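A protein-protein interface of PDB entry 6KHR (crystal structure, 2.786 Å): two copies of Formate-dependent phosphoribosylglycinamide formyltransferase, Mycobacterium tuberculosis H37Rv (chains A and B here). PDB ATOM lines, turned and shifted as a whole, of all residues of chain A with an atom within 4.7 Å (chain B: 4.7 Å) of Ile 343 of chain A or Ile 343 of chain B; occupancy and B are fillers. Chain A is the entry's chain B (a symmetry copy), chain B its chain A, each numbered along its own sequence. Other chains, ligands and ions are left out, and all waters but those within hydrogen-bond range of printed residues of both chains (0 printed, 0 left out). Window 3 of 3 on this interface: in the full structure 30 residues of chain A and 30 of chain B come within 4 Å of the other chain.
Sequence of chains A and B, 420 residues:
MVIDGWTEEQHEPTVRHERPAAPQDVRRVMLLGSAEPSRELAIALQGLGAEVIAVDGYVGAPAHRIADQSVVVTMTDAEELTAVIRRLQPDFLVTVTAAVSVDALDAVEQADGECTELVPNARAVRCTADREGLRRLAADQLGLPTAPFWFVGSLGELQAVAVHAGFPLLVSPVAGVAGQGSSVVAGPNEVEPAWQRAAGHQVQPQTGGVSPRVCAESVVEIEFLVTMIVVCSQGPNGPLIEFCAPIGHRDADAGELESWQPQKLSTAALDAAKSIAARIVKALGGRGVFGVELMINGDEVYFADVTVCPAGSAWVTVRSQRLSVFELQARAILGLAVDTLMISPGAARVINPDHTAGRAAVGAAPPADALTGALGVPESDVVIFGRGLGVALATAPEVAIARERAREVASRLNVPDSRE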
ATOM      1  N   ARG A 319      10.415 -12.425  -0.472  1.00  0.00           N
ATOM      2  CA  ARG A 319      11.644 -13.198  -0.351  1.00  0.00           C
ATOM      3  C   ARG A 319      11.807 -14.308  -1.377  1.00  0.00           C
ATOM      4  O   ARG A 319      12.934 -14.786  -1.546  1.00  0.00           O
ATOM      5  CB  ARG A 319      11.764 -13.827   1.047  1.00  0.00           C
ATOM      6  CG  ARG A 319      12.088 -12.855   2.155  1.00  0.00           C
ATOM      7  CD  ARG A 319      13.466 -12.265   1.924  1.00  0.00           C
ATOM      8  NE  ARG A 319      13.726 -11.141   2.813  1.00  0.00           N
ATOM      9  CZ  ARG A 319      14.630 -10.202   2.568  1.00  0.00           C
ATOM     10  NH1 ARG A 319      15.354 -10.264   1.457  1.00  0.00           N
ATOM     11  NH2 ARG A 319      14.810  -9.206   3.428  1.00  0.00           N
ATOM     12  N   SER A 320      10.745 -14.748  -2.053  1.00  0.00           N
ATOM     13  CA  SER A 320      10.902 -15.900  -2.941  1.00  0.00           C
ATOM     14  C   SER A 320      11.160 -15.532  -4.397  1.00  0.00           C
ATOM     15  O   SER A 320      11.615 -16.391  -5.164  1.00  0.00           O
ATOM     16  CB  SER A 320       9.676 -16.804  -2.872  1.00  0.00           C
ATOM     17  OG  SER A 320       8.496 -16.029  -2.914  1.00  0.00           O
ATOM     18  N   GLN A 321      10.895 -14.296  -4.798  1.00  0.00           N
ATOM     19  CA  GLN A 321      11.129 -13.865  -6.167  1.00  0.00           C
ATOM     20  C   GLN A 321      12.218 -12.809  -6.204  1.00  0.00           C
ATOM     21  O   GLN A 321      12.360 -12.034  -5.262  1.00  0.00           O
ATOM     22  CB  GLN A 321       9.867 -13.267  -6.814  1.00  0.00           C
ATOM     23  CG  GLN A 321       8.638 -14.133  -6.730  1.00  0.00           C
ATOM     24  CD  GLN A 321       7.599 -13.760  -7.751  1.00  0.00           C
ATOM     25  OE1 GLN A 321       7.105 -14.623  -8.466  1.00  0.00           O
ATOM     26  NE2 GLN A 321       7.257 -12.473  -7.829  1.00  0.00           N
ATOM     27  N   ARG A 322      12.963 -12.773  -7.315  1.00  0.00           N
ATOM     28  CA  ARG A 322      13.860 -11.653  -7.588  1.00  0.00           C
ATOM     29  C   ARG A 322      13.150 -10.311  -7.386  1.00  0.00           C
ATOM     30  O   ARG A 322      13.643  -9.436  -6.670  1.00  0.00           O
ATOM     31  CB  ARG A 322      14.420 -11.762  -9.006  1.00  0.00           C
ATOM     32  CG  ARG A 322      15.655 -10.928  -9.262  1.00  0.00           C
ATOM     33  CD  ARG A 322      16.091 -10.982 -10.733  1.00  0.00           C
ATOM     34  NE  ARG A 322      15.263 -10.106 -11.567  1.00  0.00           N
ATOM     35  CZ  ARG A 322      15.527  -8.828 -11.868  1.00  0.00           C
ATOM     36  NH1 ARG A 322      16.602  -8.217 -11.420  1.00  0.00           N
ATOM     37  NH2 ARG A 322      14.695  -8.160 -12.641  1.00  0.00           N
ATOM     38  N   LEU A 341      11.406 -14.211 -12.375  1.00  0.00           N
ATOM     39  CA  LEU A 341      12.354 -15.178 -11.825  1.00  0.00           C
ATOM     40  C   LEU A 341      12.165 -15.380 -10.327  1.00  0.00           C
ATOM     41  O   LEU A 341      11.955 -14.425  -9.577  1.00  0.00           O
ATOM     42  CB  LEU A 341      13.790 -14.714 -12.093  1.00  0.00           C
ATOM     43  CG  LEU A 341      14.115 -14.315 -13.536  1.00  0.00           C
ATOM     44  CD1 LEU A 341      15.474 -13.615 -13.617  1.00  0.00           C
ATOM     45  CD2 LEU A 341      14.069 -15.522 -14.454  1.00  0.00           C
ATOM     46  N   MET A 342      12.296 -16.631  -9.893  1.00  0.00           N
ATOM     47  CA  MET A 342      12.255 -17.012  -8.486  1.00  0.00           C
ATOM     48  C   MET A 342      13.653 -17.128  -7.886  1.00  0.00           C
ATOM     49  O   MET A 342      14.562 -17.706  -8.497  1.00  0.00           O
ATOM     50  CB  MET A 342      11.523 -18.346  -8.306  1.00  0.00           C
ATOM     51  CG  MET A 342      10.051 -18.232  -8.567  1.00  0.00           C
ATOM     52  SD  MET A 342       9.088 -19.496  -7.755  1.00  0.00           S
ATOM     53  CE  MET A 342       9.571 -19.337  -6.032  1.00  0.00           C
ATOM     54  N   ILE A 343      13.814 -16.594  -6.676  1.00  0.00           N
ATOM     55  CA  ILE A 343      15.054 -16.797  -5.932  1.00  0.00           C
ATOM     56  C   ILE A 343      15.146 -18.241  -5.441  1.00  0.00           C
ATOM     57  O   ILE A 343      16.160 -18.920  -5.631  1.00  0.00           O
ATOM     58  CB  ILE A 343      15.126 -15.815  -4.747  1.00  0.00           C
ATOM     59  CG1 ILE A 343      15.261 -14.366  -5.217  1.00  0.00           C
ATOM     60  CG2 ILE A 343      16.290 -16.172  -3.819  1.00  0.00           C
ATOM     61  CD1 ILE A 343      15.126 -13.373  -4.037  1.00  0.00           C
ATOM     62  N   SER A 344      14.084 -18.732  -4.815  1.00  0.00           N
ATOM     63  CA  SER A 344      14.103 -19.972  -4.056  1.00  0.00           C
ATOM     64  C   SER A 344      12.683 -20.239  -3.558  1.00  0.00           C
ATOM     65  O   SER A 344      11.882 -19.308  -3.448  1.00  0.00           O
ATOM     66  CB  SER A 344      15.088 -19.880  -2.878  1.00  0.00           C
ATOM     67  OG  SER A 344      14.543 -20.436  -1.697  1.00  0.00           O
ATOM     68  N   ARG B 319      21.112  -6.673  -4.154  1.00  0.00           N
ATOM     69  CA  ARG B 319      20.569  -7.715  -5.017  1.00  0.00           C
ATOM     70  C   ARG B 319      21.327  -9.033  -4.989  1.00  0.00           C
ATOM     71  O   ARG B 319      20.765 -10.042  -5.428  1.00  0.00           O
ATOM     72  CB  ARG B 319      20.507  -7.242  -6.481  1.00  0.00           C
ATOM     73  CG  ARG B 319      19.428  -6.225  -6.775  1.00  0.00           C
ATOM     74  CD  ARG B 319      18.067  -6.858  -6.558  1.00  0.00           C
ATOM     75  NE  ARG B 319      17.005  -5.866  -6.580  1.00  0.00           N
ATOM     76  CZ  ARG B 319      15.814  -6.048  -6.023  1.00  0.00           C
ATOM     77  NH1 ARG B 319      15.546  -7.192  -5.405  1.00  0.00           N
ATOM     78  NH2 ARG B 319      14.893  -5.091  -6.083  1.00  0.00           N
ATOM     79  N   SER B 320      22.571  -9.072  -4.510  1.00  0.00           N
ATOM     80  CA  SER B 320      23.326 -10.323  -4.605  1.00  0.00           C
ATOM     81  C   SER B 320      23.258 -11.185  -3.352  1.00  0.00           C
ATOM     82  O   SER B 320      23.580 -12.378  -3.424  1.00  0.00           O
ATOM     83  CB  SER B 320      24.789 -10.045  -4.931  1.00  0.00           C
ATOM     84  OG  SER B 320      25.274  -8.981  -4.137  1.00  0.00           O
ATOM     85  N   GLN B 321      22.845 -10.633  -2.219  1.00  0.00           N
ATOM     86  CA  GLN B 321      22.738 -11.399  -0.985  1.00  0.00           C
ATOM     87  C   GLN B 321      21.287 -11.496  -0.555  1.00  0.00           C
ATOM     88  O   GLN B 321      20.504 -10.586  -0.808  1.00  0.00           O
ATOM     89  CB  GLN B 321      23.532 -10.757   0.167  1.00  0.00           C
ATOM     90  CG  GLN B 321      24.972 -10.448  -0.146  1.00  0.00           C
ATOM     91  CD  GLN B 321      25.811 -10.290   1.092  1.00  0.00           C
ATOM     92  OE1 GLN B 321      26.862 -10.903   1.203  1.00  0.00           O
ATOM     93  NE2 GLN B 321      25.352  -9.464   2.036  1.00  0.00           N
ATOM     94  N   ARG B 322      20.948 -12.604   0.118  1.00  0.00           N
ATOM     95  CA  ARG B 322      19.665 -12.702   0.809  1.00  0.00           C
ATOM     96  C   ARG B 322      19.396 -11.462   1.663  1.00  0.00           C
ATOM     97  O   ARG B 322      18.334 -10.844   1.563  1.00  0.00           O
ATOM     98  CB  ARG B 322      19.630 -13.972   1.665  1.00  0.00           C
ATOM     99  CG  ARG B 322      18.242 -14.406   2.084  1.00  0.00           C
ATOM    100  CD  ARG B 322      18.282 -15.608   3.043  1.00  0.00           C
ATOM    101  NE  ARG B 322      18.619 -15.188   4.406  1.00  0.00           N
ATOM    102  CZ  ARG B 322      17.748 -14.859   5.366  1.00  0.00           C
ATOM    103  NH1 ARG B 322      16.447 -14.879   5.163  1.00  0.00           N
ATOM    104  NH2 ARG B 322      18.194 -14.507   6.557  1.00  0.00           N
ATOM    105  N   LEU B 341      24.198 -15.617   3.353  1.00  0.00           N
ATOM    106  CA  LEU B 341      23.883 -16.331   2.118  1.00  0.00           C
ATOM    107  C   LEU B 341      23.793 -15.389   0.920  1.00  0.00           C
ATOM    108  O   LEU B 341      23.228 -14.298   1.007  1.00  0.00           O
ATOM    109  CB  LEU B 341      22.561 -17.080   2.266  1.00  0.00           C
ATOM    110  CG  LEU B 341      22.418 -17.962   3.514  1.00  0.00           C
ATOM    111  CD1 LEU B 341      20.972 -18.433   3.692  1.00  0.00           C
ATOM    112  CD2 LEU B 341      23.370 -19.144   3.453  1.00  0.00           C
ATOM    113  N   MET B 342      24.312 -15.851  -0.213  1.00  0.00           N
ATOM    114  CA  MET B 342      24.228 -15.148  -1.490  1.00  0.00           C
ATOM    115  C   MET B 342      23.062 -15.645  -2.340  1.00  0.00           C
ATOM    116  O   MET B 342      22.830 -16.855  -2.460  1.00  0.00           O
ATOM    117  CB  MET B 342      25.528 -15.314  -2.285  1.00  0.00           C
ATOM    118  CG  MET B 342      26.673 -14.565  -1.673  1.00  0.00           C
ATOM    119  SD  MET B 342      27.965 -14.167  -2.839  1.00  0.00           S
ATOM    120  CE  MET B 342      27.087 -13.287  -4.136  1.00  0.00           C
ATOM    121  N   ILE B 343      22.341 -14.703  -2.945  1.00  0.00           N
ATOM    122  CA  ILE B 343      21.311 -15.061  -3.919  1.00  0.00           C
ATOM    123  C   ILE B 343      21.957 -15.569  -5.207  1.00  0.00           C
ATOM    124  O   ILE B 343      21.604 -16.630  -5.729  1.00  0.00           O
ATOM    125  CB  ILE B 343      20.407 -13.846  -4.204  1.00  0.00           C
ATOM    126  CG1 ILE B 343      19.575 -13.457  -2.980  1.00  0.00           C
ATOM    127  CG2 ILE B 343      19.483 -14.128  -5.393  1.00  0.00           C
ATOM    128  CD1 ILE B 343      18.827 -12.124  -3.209  1.00  0.00           C
ATOM    129  N   SER B 344      22.922 -14.821  -5.728  1.00  0.00           N
ATOM    130  CA  SER B 344      23.442 -15.009  -7.073  1.00  0.00           C
ATOM    131  C   SER B 344      24.589 -14.016  -7.278  1.00  0.00           C
ATOM    132  O   SER B 344      24.648 -12.995  -6.587  1.00  0.00           O
ATOM    133  CB  SER B 344      22.344 -14.794  -8.124  1.00  0.00           C
ATOM    134  OG  SER B 344      22.808 -14.036  -9.223  1.00  0.00           O
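Arg 319 of chain A touches Arg 322 of chain B, and with the chains exchanged Arg 322 of chain A touches Arg 319 of chain B.
Ile 343 of chain A touches its own counterpart, Ile 343 of chain B.
O of Arg 322 of chain A lies within hydrogen-bond range of NH1 of Arg 319 of chain B, at 3.2 Å.
NH1 of Arg 319 of chain A lies within hydrogen-bond range of O of Arg 322 of chain B, 3.0 Å away.
Hydrophobic or aromatic side chains of chain A within 4 Å of the printed part of chain B: Ile 343.
Printed residues of chain B that touch a printed residue of chain A: Arg 319, Arg 322 and Ile 343.
Along chain B the printed residues that touch a printed residue of chain A span positions 319 to 343.
The backbone carbonyl oxygen of Ser 320 of chain B is in hydrogen-bond range of the backbone NH of Ile 343 of chain B (2.7 Å).
N of Arg 322 of chain B sits at hydrogen-bond distance from O of Leu 341 of chain B (3.0 Å).
O of Ser 320 of chain A is in hydrogen-bond range of N of Ile 343 of chain A.
The backbone NH (N) of Arg 322 of chain A lies within hydrogen-bond range of the backbone carbonyl oxygen (O) of Leu 341 of chain A (3.0 Å).
Printed residues of chain B within 4 Å of Arg 319 of chain A: Arg 322 (3.0 Å).
Ser 320 of chain A touches none of the printed residues of chain B.
Printed residues of chain B within 4 Å of Arg 322 of chain A: Arg 319.
Printed residues of chain B within 4 Å of Ile 343 of chain A: Ile 343.
Printed residues of chain A within 4 Å of Arg 319 of chain B: Arg 322 (3.2 Å).
Printed residues of chain A within 4 Å of Arg 322 of chain B: Arg 319 (3.0 Å).
Met 342 of chain B touches none of the printed residues of chain A.
Of the printed residues of chain A, Ile 343 of chain B touches Ile 343 (3.99 Å).
The nearest printed residue of chain B that does not touch Ile 343 of chain A is Arg 319 of chain B (6.3 Å).
Among the printed residues, merely in contact across the chains: Ile 343 of chain A with Ile 343 of chain B.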
